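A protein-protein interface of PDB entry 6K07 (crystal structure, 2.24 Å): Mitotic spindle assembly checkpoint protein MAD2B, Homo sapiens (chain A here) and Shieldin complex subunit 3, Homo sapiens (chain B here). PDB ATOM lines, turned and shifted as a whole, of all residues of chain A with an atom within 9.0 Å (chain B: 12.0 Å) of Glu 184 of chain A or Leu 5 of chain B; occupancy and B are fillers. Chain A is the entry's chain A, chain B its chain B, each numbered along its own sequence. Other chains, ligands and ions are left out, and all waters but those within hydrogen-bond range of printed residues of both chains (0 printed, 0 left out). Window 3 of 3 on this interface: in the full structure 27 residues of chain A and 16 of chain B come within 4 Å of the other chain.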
ATOM      1  N   LEU A  96     -16.732 -21.274  22.639  1.00  0.00           N
ATOM      2  CA  LEU A  96     -16.172 -22.612  22.487  1.00  0.00           C
ATOM      3  C   LEU A  96     -14.941 -22.587  21.583  1.00  0.00           C
ATOM      4  O   LEU A  96     -14.865 -21.786  20.651  1.00  0.00           O
ATOM      5  CB  LEU A  96     -17.238 -23.565  21.923  1.00  0.00           C
ATOM      6  CG  LEU A  96     -18.540 -23.544  22.732  1.00  0.00           C
ATOM      7  CD1 LEU A  96     -19.557 -24.502  22.178  1.00  0.00           C
ATOM      8  CD2 LEU A  96     -18.257 -23.903  24.179  1.00  0.00           C
ATOM      9  N   HIS A 100     -14.933 -27.707  20.617  1.00  0.00           N
ATOM     10  CA  HIS A 100     -16.230 -27.717  21.310  1.00  0.00           C
ATOM     11  C   HIS A 100     -16.069 -27.816  22.823  1.00  0.00           C
ATOM     12  O   HIS A 100     -16.823 -28.521  23.498  1.00  0.00           O
ATOM     13  CB  HIS A 100     -17.135 -28.850  20.822  1.00  0.00           C
ATOM     14  CG  HIS A 100     -17.065 -29.108  19.347  1.00  0.00           C
ATOM     15  ND1 HIS A 100     -16.365 -30.170  18.812  1.00  0.00           N
ATOM     16  CD2 HIS A 100     -17.641 -28.468  18.299  1.00  0.00           C
ATOM     17  CE1 HIS A 100     -16.494 -30.160  17.497  1.00  0.00           C
ATOM     18  NE2 HIS A 100     -17.260 -29.135  17.160  1.00  0.00           N
ATOM     19  N   ARG A 101     -15.065 -27.132  23.361  1.00  0.00           N
ATOM     20  CA  ARG A 101     -14.901 -27.032  24.801  1.00  0.00           C
ATOM     21  C   ARG A 101     -15.012 -25.568  25.211  1.00  0.00           C
ATOM     22  O   ARG A 101     -14.518 -24.695  24.491  1.00  0.00           O
ATOM     23  CB  ARG A 101     -13.545 -27.613  25.260  1.00  0.00           C
ATOM     24  N   PRO A 102     -15.682 -25.262  26.325  1.00  0.00           N
ATOM     25  CA  PRO A 102     -15.860 -23.847  26.711  1.00  0.00           C
ATOM     26  C   PRO A 102     -14.539 -23.229  27.149  1.00  0.00           C
ATOM     27  O   PRO A 102     -13.814 -23.813  27.946  1.00  0.00           O
ATOM     28  CB  PRO A 102     -16.869 -23.913  27.871  1.00  0.00           C
ATOM     29  CG  PRO A 102     -17.404 -25.327  27.869  1.00  0.00           C
ATOM     30  CD  PRO A 102     -16.343 -26.184  27.262  1.00  0.00           C
ATOM     31  N   LYS A 105     -17.065 -18.102  29.762  1.00  0.00           N
ATOM     32  CA  LYS A 105     -18.495 -17.918  29.940  1.00  0.00           C
ATOM     33  C   LYS A 105     -18.711 -16.464  30.318  1.00  0.00           C
ATOM     34  O   LYS A 105     -17.992 -15.933  31.168  1.00  0.00           O
ATOM     35  CB  LYS A 105     -19.049 -18.860  31.025  1.00  0.00           C
ATOM     36  CG  LYS A 105     -19.100 -20.344  30.637  1.00  0.00           C
ATOM     37  CD  LYS A 105     -19.347 -21.206  31.870  1.00  0.00           C
ATOM     38  CE  LYS A 105     -20.346 -22.333  31.594  1.00  0.00           C
ATOM     39  NZ  LYS A 105     -21.578 -22.268  32.483  1.00  0.00           N
ATOM     40  N   LEU A 157     -26.572 -20.197  26.655  1.00  0.00           N
ATOM     41  CA  LEU A 157     -27.214 -21.114  27.570  1.00  0.00           C
ATOM     42  C   LEU A 157     -28.165 -20.343  28.467  1.00  0.00           C
ATOM     43  O   LEU A 157     -27.832 -19.269  28.977  1.00  0.00           O
ATOM     44  CB  LEU A 157     -26.178 -21.847  28.405  1.00  0.00           C
ATOM     45  CG  LEU A 157     -24.992 -22.372  27.613  1.00  0.00           C
ATOM     46  CD1 LEU A 157     -23.855 -22.528  28.606  1.00  0.00           C
ATOM     47  CD2 LEU A 157     -25.334 -23.700  26.927  1.00  0.00           C
ATOM     48  N   VAL A 158     -29.346 -20.900  28.663  1.00  0.00           N
ATOM     49  CA  VAL A 158     -30.351 -20.315  29.535  1.00  0.00           C
ATOM     50  C   VAL A 158     -30.528 -21.251  30.724  1.00  0.00           C
ATOM     51  O   VAL A 158     -30.802 -22.443  30.543  1.00  0.00           O
ATOM     52  CB  VAL A 158     -31.667 -20.077  28.778  1.00  0.00           C
ATOM     53  CG1 VAL A 158     -32.783 -19.672  29.723  1.00  0.00           C
ATOM     54  CG2 VAL A 158     -31.444 -19.011  27.728  1.00  0.00           C
ATOM     55  N   HIS A 159     -30.315 -20.724  31.933  1.00  0.00           N
ATOM     56  CA  HIS A 159     -30.601 -21.430  33.178  1.00  0.00           C
ATOM     57  C   HIS A 159     -31.907 -20.893  33.745  1.00  0.00           C
ATOM     58  O   HIS A 159     -32.009 -19.691  34.025  1.00  0.00           O
ATOM     59  CB  HIS A 159     -29.486 -21.226  34.209  1.00  0.00           C
ATOM     60  CG  HIS A 159     -28.159 -21.817  33.830  1.00  0.00           C
ATOM     61  ND1 HIS A 159     -27.675 -22.985  34.383  1.00  0.00           N
ATOM     62  CD2 HIS A 159     -27.195 -21.376  32.984  1.00  0.00           C
ATOM     63  CE1 HIS A 159     -26.481 -23.248  33.880  1.00  0.00           C
ATOM     64  NE2 HIS A 159     -26.164 -22.284  33.031  1.00  0.00           N
ATOM     65  N   THR A 160     -32.886 -21.777  33.943  1.00  0.00           N
ATOM     66  CA  THR A 160     -34.201 -21.419  34.465  1.00  0.00           C
ATOM     67  C   THR A 160     -34.273 -21.658  35.973  1.00  0.00           C
ATOM     68  O   THR A 160     -33.522 -22.460  36.533  1.00  0.00           O
ATOM     69  CB  THR A 160     -35.301 -22.227  33.773  1.00  0.00           C
ATOM     70  OG1 THR A 160     -34.873 -23.590  33.621  1.00  0.00           O
ATOM     71  CG2 THR A 160     -35.595 -21.650  32.428  1.00  0.00           C
ATOM     72  N   ASN A 167     -40.240 -25.638  30.308  1.00  0.00           N
ATOM     73  CA  ASN A 167     -39.468 -24.586  29.677  1.00  0.00           C
ATOM     74  C   ASN A 167     -39.249 -24.897  28.211  1.00  0.00           C
ATOM     75  O   ASN A 167     -39.378 -24.018  27.359  1.00  0.00           O
ATOM     76  CB  ASN A 167     -38.148 -24.422  30.412  1.00  0.00           C
ATOM     77  CG  ASN A 167     -38.350 -23.954  31.830  1.00  0.00           C
ATOM     78  OD1 ASN A 167     -37.651 -24.398  32.748  1.00  0.00           O
ATOM     79  ND2 ASN A 167     -39.307 -23.044  32.022  1.00  0.00           N
ATOM     80  N   MET A 168     -38.968 -26.155  27.891  1.00  0.00           N
ATOM     81  CA  MET A 168     -38.779 -26.493  26.491  1.00  0.00           C
ATOM     82  C   MET A 168     -40.064 -26.390  25.684  1.00  0.00           C
ATOM     83  O   MET A 168     -40.017 -26.568  24.466  1.00  0.00           O
ATOM     84  CB  MET A 168     -38.184 -27.883  26.331  1.00  0.00           C
ATOM     85  CG  MET A 168     -36.679 -27.838  26.366  1.00  0.00           C
ATOM     86  SD  MET A 168     -35.825 -29.200  25.551  1.00  0.00           S
ATOM     87  CE  MET A 168     -36.953 -29.604  24.212  1.00  0.00           C
ATOM     88  N   ILE A 180     -32.739 -27.260  22.978  1.00  0.00           N
ATOM     89  CA  ILE A 180     -32.516 -28.579  23.558  1.00  0.00           C
ATOM     90  C   ILE A 180     -31.935 -28.401  24.951  1.00  0.00           C
ATOM     91  O   ILE A 180     -31.658 -27.286  25.397  1.00  0.00           O
ATOM     92  CB  ILE A 180     -31.584 -29.461  22.701  1.00  0.00           C
ATOM     93  CG1 ILE A 180     -30.181 -28.856  22.646  1.00  0.00           C
ATOM     94  CG2 ILE A 180     -32.143 -29.626  21.315  1.00  0.00           C
ATOM     95  CD1 ILE A 180     -29.338 -29.364  21.493  1.00  0.00           C
ATOM     96  N   LEU A 181     -31.738 -29.520  25.625  1.00  0.00           N
ATOM     97  CA  LEU A 181     -30.945 -29.537  26.837  1.00  0.00           C
ATOM     98  C   LEU A 181     -29.466 -29.619  26.479  1.00  0.00           C
ATOM     99  O   LEU A 181     -29.058 -30.462  25.671  1.00  0.00           O
ATOM    100  CB  LEU A 181     -31.346 -30.720  27.698  1.00  0.00           C
ATOM    101  CG  LEU A 181     -31.024 -30.525  29.164  1.00  0.00           C
ATOM    102  CD1 LEU A 181     -31.720 -29.285  29.658  1.00  0.00           C
ATOM    103  CD2 LEU A 181     -31.503 -31.748  29.906  1.00  0.00           C
ATOM    104  N   ALA A 182     -28.668 -28.729  27.062  1.00  0.00           N
ATOM    105  CA  ALA A 182     -27.232 -28.785  26.835  1.00  0.00           C
ATOM    106  C   ALA A 182     -26.644 -30.036  27.483  1.00  0.00           C
ATOM    107  O   ALA A 182     -27.220 -30.616  28.407  1.00  0.00           O
ATOM    108  CB  ALA A 182     -26.539 -27.543  27.393  1.00  0.00           C
ATOM    109  N   ASP A 183     -25.490 -30.456  26.972  1.00  0.00           N
ATOM    110  CA  ASP A 183     -24.709 -31.534  27.552  1.00  0.00           C
ATOM    111  C   ASP A 183     -23.729 -30.970  28.576  1.00  0.00           C
ATOM    112  O   ASP A 183     -23.516 -29.758  28.669  1.00  0.00           O
ATOM    113  CB  ASP A 183     -23.957 -32.300  26.468  1.00  0.00           C
ATOM    114  CG  ASP A 183     -24.840 -32.661  25.302  1.00  0.00           C
ATOM    115  OD1 ASP A 183     -25.368 -31.719  24.659  1.00  0.00           O
ATOM    116  OD2 ASP A 183     -24.993 -33.875  25.023  1.00  0.00           O
ATOM    117  N   GLU A 184     -23.127 -31.876  29.356  1.00  0.00           N
ATOM    118  CA  GLU A 184     -22.128 -31.454  30.332  1.00  0.00           C
ATOM    119  C   GLU A 184     -20.903 -30.869  29.648  1.00  0.00           C
ATOM    120  O   GLU A 184     -20.261 -29.971  30.199  1.00  0.00           O
ATOM    121  CB  GLU A 184     -21.725 -32.624  31.233  1.00  0.00           C
ATOM    122  N   GLN A 185     -20.567 -31.359  28.452  1.00  0.00           N
ATOM    123  CA  GLN A 185     -19.431 -30.801  27.729  1.00  0.00           C
ATOM    124  C   GLN A 185     -19.722 -29.387  27.246  1.00  0.00           C
ATOM    125  O   GLN A 185     -18.800 -28.572  27.127  1.00  0.00           O
ATOM    126  CB  GLN A 185     -19.056 -31.713  26.561  1.00  0.00           C
ATOM    127  CG  GLN A 185     -17.893 -31.216  25.723  1.00  0.00           C
ATOM    128  CD  GLN A 185     -17.494 -32.213  24.657  1.00  0.00           C
ATOM    129  OE1 GLN A 185     -18.096 -32.255  23.579  1.00  0.00           O
ATOM    130  NE2 GLN A 185     -16.479 -33.029  24.951  1.00  0.00           N
ATOM    131  N   ASP A 186     -20.995 -29.064  26.992  1.00  0.00           N
ATOM    132  CA  ASP A 186     -21.359 -27.713  26.572  1.00  0.00           C
ATOM    133  C   ASP A 186     -21.026 -26.663  27.623  1.00  0.00           C
ATOM    134  O   ASP A 186     -20.993 -25.470  27.293  1.00  0.00           O
ATOM    135  CB  ASP A 186     -22.855 -27.639  26.263  1.00  0.00           C
ATOM    136  CG  ASP A 186     -23.186 -28.093  24.862  1.00  0.00           C
ATOM    137  OD1 ASP A 186     -22.248 -28.193  24.043  1.00  0.00           O
ATOM    138  OD2 ASP A 186     -24.382 -28.353  24.586  1.00  0.00           O
ATOM    139  N   VAL A 187     -20.809 -27.066  28.882  1.00  0.00           N
ATOM    140  CA  VAL A 187     -20.767 -26.114  29.989  1.00  0.00           C
ATOM    141  C   VAL A 187     -19.649 -26.428  30.970  1.00  0.00           C
ATOM    142  O   VAL A 187     -19.440 -25.674  31.925  1.00  0.00           O
ATOM    143  CB  VAL A 187     -22.117 -26.058  30.740  1.00  0.00           C
ATOM    144  CG1 VAL A 187     -23.275 -25.877  29.776  1.00  0.00           C
ATOM    145  CG2 VAL A 187     -22.327 -27.310  31.584  1.00  0.00           C
ATOM    146  N   HIS A 188     -18.929 -27.532  30.754  1.00  0.00           N
ATOM    147  CA  HIS A 188     -17.949 -27.997  31.736  1.00  0.00           C
ATOM    148  C   HIS A 188     -16.745 -27.064  31.798  1.00  0.00           C
ATOM    149  O   HIS A 188     -16.114 -26.773  30.777  1.00  0.00           O
ATOM    150  CB  HIS A 188     -17.485 -29.424  31.414  1.00  0.00           C
ATOM    151  CG  HIS A 188     -16.523 -29.993  32.418  1.00  0.00           C
ATOM    152  ND1 HIS A 188     -16.607 -29.721  33.769  1.00  0.00           N
ATOM    153  CD2 HIS A 188     -15.457 -30.814  32.267  1.00  0.00           C
ATOM    154  CE1 HIS A 188     -15.636 -30.352  34.404  1.00  0.00           C
ATOM    155  NE2 HIS A 188     -14.923 -31.022  33.516  1.00  0.00           N
ATOM    156  N   MET A 189     -16.401 -26.625  33.009  1.00  0.00           N
ATOM    157  CA  MET A 189     -15.275 -25.715  33.178  1.00  0.00           C
ATOM    158  C   MET A 189     -14.707 -25.908  34.586  1.00  0.00           C
ATOM    159  O   MET A 189     -15.005 -25.151  35.510  1.00  0.00           O
ATOM    160  CB  MET A 189     -15.708 -24.272  32.946  1.00  0.00           C
ATOM    161  CG  MET A 189     -14.579 -23.334  32.640  1.00  0.00           C
ATOM    162  SD  MET A 189     -15.244 -21.856  31.873  1.00  0.00           S
ATOM    163  CE  MET A 189     -14.920 -22.183  30.174  1.00  0.00           C
ATOM    164  N   HIS A 190     -13.879 -26.941  34.748  1.00  0.00           N
ATOM    165  CA  HIS A 190     -13.310 -27.233  36.061  1.00  0.00           C
ATOM    166  C   HIS A 190     -12.389 -26.098  36.503  1.00  0.00           C
ATOM    167  O   HIS A 190     -11.468 -25.711  35.775  1.00  0.00           O
ATOM    168  CB  HIS A 190     -12.550 -28.564  36.048  1.00  0.00           C
ATOM    169  N   LEU B   5     -28.775 -28.545  34.450  1.00  0.00           N
ATOM    170  CA  LEU B   5     -28.178 -28.400  33.118  1.00  0.00           C
ATOM    171  C   LEU B   5     -29.036 -27.521  32.195  1.00  0.00           C
ATOM    172  O   LEU B   5     -30.206 -27.795  31.977  1.00  0.00           O
ATOM    173  CB  LEU B   5     -27.954 -29.776  32.482  1.00  0.00           C
ATOM    174  CG  LEU B   5     -26.619 -29.970  31.748  1.00  0.00           C
ATOM    175  CD1 LEU B   5     -25.471 -29.519  32.626  1.00  0.00           C
ATOM    176  CD2 LEU B   5     -26.421 -31.417  31.355  1.00  0.00           C
ATOM    177  N   PRO B   6     -28.449 -26.479  31.632  1.00  0.00           N
ATOM    178  CA  PRO B   6     -29.236 -25.448  30.951  1.00  0.00           C
ATOM    179  C   PRO B   6     -29.753 -25.896  29.583  1.00  0.00           C
ATOM    180  O   PRO B   6     -29.462 -26.985  29.078  1.00  0.00           O
ATOM    181  CB  PRO B   6     -28.245 -24.286  30.811  1.00  0.00           C
ATOM    182  CG  PRO B   6     -26.917 -24.937  30.753  1.00  0.00           C
ATOM    183  CD  PRO B   6     -27.009 -26.171  31.629  1.00  0.00           C
ATOM    184  N   LEU B   7     -30.555 -25.011  28.999  1.00  0.00           N
ATOM    185  CA  LEU B   7     -31.043 -25.126  27.641  1.00  0.00           C
ATOM    186  C   LEU B   7     -30.182 -24.281  26.720  1.00  0.00           C
ATOM    187  O   LEU B   7     -29.624 -23.248  27.119  1.00  0.00           O
ATOM    188  CB  LEU B   7     -32.488 -24.652  27.522  1.00  0.00           C
ATOM    189  CG  LEU B   7     -33.559 -25.365  28.333  1.00  0.00           C
ATOM    190  CD1 LEU B   7     -34.913 -24.679  28.170  1.00  0.00           C
ATOM    191  CD2 LEU B   7     -33.632 -26.776  27.876  1.00  0.00           C
ATOM    192  N   ARG B   8     -30.099 -24.721  25.475  1.00  0.00           N
ATOM    193  CA  ARG B   8     -29.400 -23.983  24.440  1.00  0.00           C
ATOM    194  C   ARG B   8     -30.162 -24.166  23.142  1.00  0.00           C
ATOM    195  O   ARG B   8     -30.983 -25.082  23.015  1.00  0.00           O
ATOM    196  CB  ARG B   8     -27.945 -24.454  24.294  1.00  0.00           C
ATOM    197  CG  ARG B   8     -27.796 -25.885  23.867  1.00  0.00           C
ATOM    198  CD  ARG B   8     -26.543 -26.090  23.035  1.00  0.00           C
ATOM    199  NE  ARG B   8     -26.518 -27.436  22.461  1.00  0.00           N
ATOM    200  CZ  ARG B   8     -25.618 -27.863  21.578  1.00  0.00           C
ATOM    201  NH1 ARG B   8     -24.663 -27.041  21.164  1.00  0.00           N
ATOM    202  NH2 ARG B   8     -25.672 -29.110  21.113  1.00  0.00           N
ATOM    203  N   PRO B   9     -29.939 -23.297  22.172  1.00  0.00           N
ATOM    204  CA  PRO B   9     -30.536 -23.526  20.860  1.00  0.00           C
ATOM    205  C   PRO B   9     -29.939 -24.770  20.237  1.00  0.00           C
ATOM    206  O   PRO B   9     -28.744 -25.031  20.374  1.00  0.00           O
ATOM    207  CB  PRO B   9     -30.175 -22.255  20.076  1.00  0.00           C
ATOM    208  CG  PRO B   9     -29.841 -21.225  21.146  1.00  0.00           C
ATOM    209  CD  PRO B   9     -29.202 -22.020  22.233  1.00  0.00           C
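The backbone NH of Val 158 of chain A lies within hydrogen-bond range of the backbone carbonyl oxygen of Leu 7 of chain B.
The backbone NH (N) of Ala 182 of chain A is in hydrogen-bond range of the backbone carbonyl oxygen (O) of Pro 6 of chain B, at 2.8 Å.
N of Ile 180 of chain A sits at hydrogen-bond distance from O of Arg 8 of chain B.
OD2 of Asp 186 of chain A is in salt-bridge range of NE of Arg 8 of chain B, 3.1 Å away.
The backbone NH of Asp 183 of chain A is in hydrogen-bond range of the side-chain carboxylate of Asp 186 of chain A.
The side-chain hydroxyl (OG1) of Thr 160 of chain A lies within hydrogen-bond range of the side-chain amide oxygen (OD1) of Asn 167 of chain A, at 3.0 Å.
Leu 157 of chain A touches Leu 7 of chain B (CA to O, 3.3 Å).
O of Val 158 of chain A touches CB of Pro 6 of chain B, at 3.2 Å.
NE2 of His 159 of chain A touches CG of Pro 6 of chain B, 3.6 Å away.
Asn 167 of chain A touches Leu 7 of chain B (CB to CD1, 3.9 Å).
Met 168 of chain A touches Leu 7 of chain B.
Leu 181 of chain A touches Leu 5 of chain B.
Ala 182 of chain A touches Leu 5 of chain B (O to CD2, 3.2 Å).
CD2 of Leu 5 of chain B touches C of Asp 183 of chain A (3.9 Å).
CG2 of Val 187 of chain A touches CD1 of Leu 5 of chain B, 3.98 Å away.
Val 187 of chain A touches Pro 6 of chain B (CG1 to CG, 3.9 Å).
Printed residues of chain A within 4 Å of Leu 5 of chain B: Leu 181, Ala 182, Asp 183, Glu 184 and Val 187.
Leu 181 of chain A touches just these residues of chain B: Leu 5, Pro 6 and Leu 7.
Of the printed residues of chain B, Ala 182 of chain A touches Leu 5 (3.2 Å) and Pro 6 (2.8 Å).
Of chain B, only Leu 5 (3.9 Å) comes within 4 Å of Asp 183 of chain A.
Gln 185 of chain A touches none of the printed residues of chain B.
Of chain B, only Arg 8 (3.1 Å) comes within 4 Å of Asp 186 of chain A.
Of the printed residues of chain A, Pro 6 of chain B touches Leu 157, Val 158, His 159, Leu 181, Ala 182 and Val 187.
Printed residues of chain A within 4 Å of Leu 7 of chain B: Leu 157, Val 158, Asn 167, Met 168, Ile 180 and Leu 181.
Of the printed residues of chain B, His 159 of chain A touches Pro 6 (3.6 Å).
Printed residues of chain B within 4 Å of Val 187 of chain A: Leu 5 and Pro 6.
Of the printed residues of chain B, Asn 167 of chain A touches Leu 7.
Pro 9 of chain B touches none of the printed residues of chain A.
Thr 160 of chain A touches none of the printed residues of chain B.
The nearest printed residue of chain A that does not touch Leu 5 of chain B is His 159 of chain A (5.2 Å).
Hydrophobic or aromatic side chains of chain A within 4 Å of the printed part of chain B: Leu 157, His 159, Met 168, Ile 180, Leu 181, Ala 182 and Val 187.
Of the 5 printed residues of chain B, 4 touch a printed residue of chain A.
Hydrophobic or aromatic side chains of chain B that line the printed part of chain A: Leu 5, Pro 6 and Leu 7.
Among the printed residues, 20 pairs touch across the chains.
Among the printed residues, Asp or Glu carboxylates within 4 Å of a Lys or Arg side-chain nitrogen of the other chain: Asp 186 of chain A with Arg 8 of chain B (3.1 Å).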
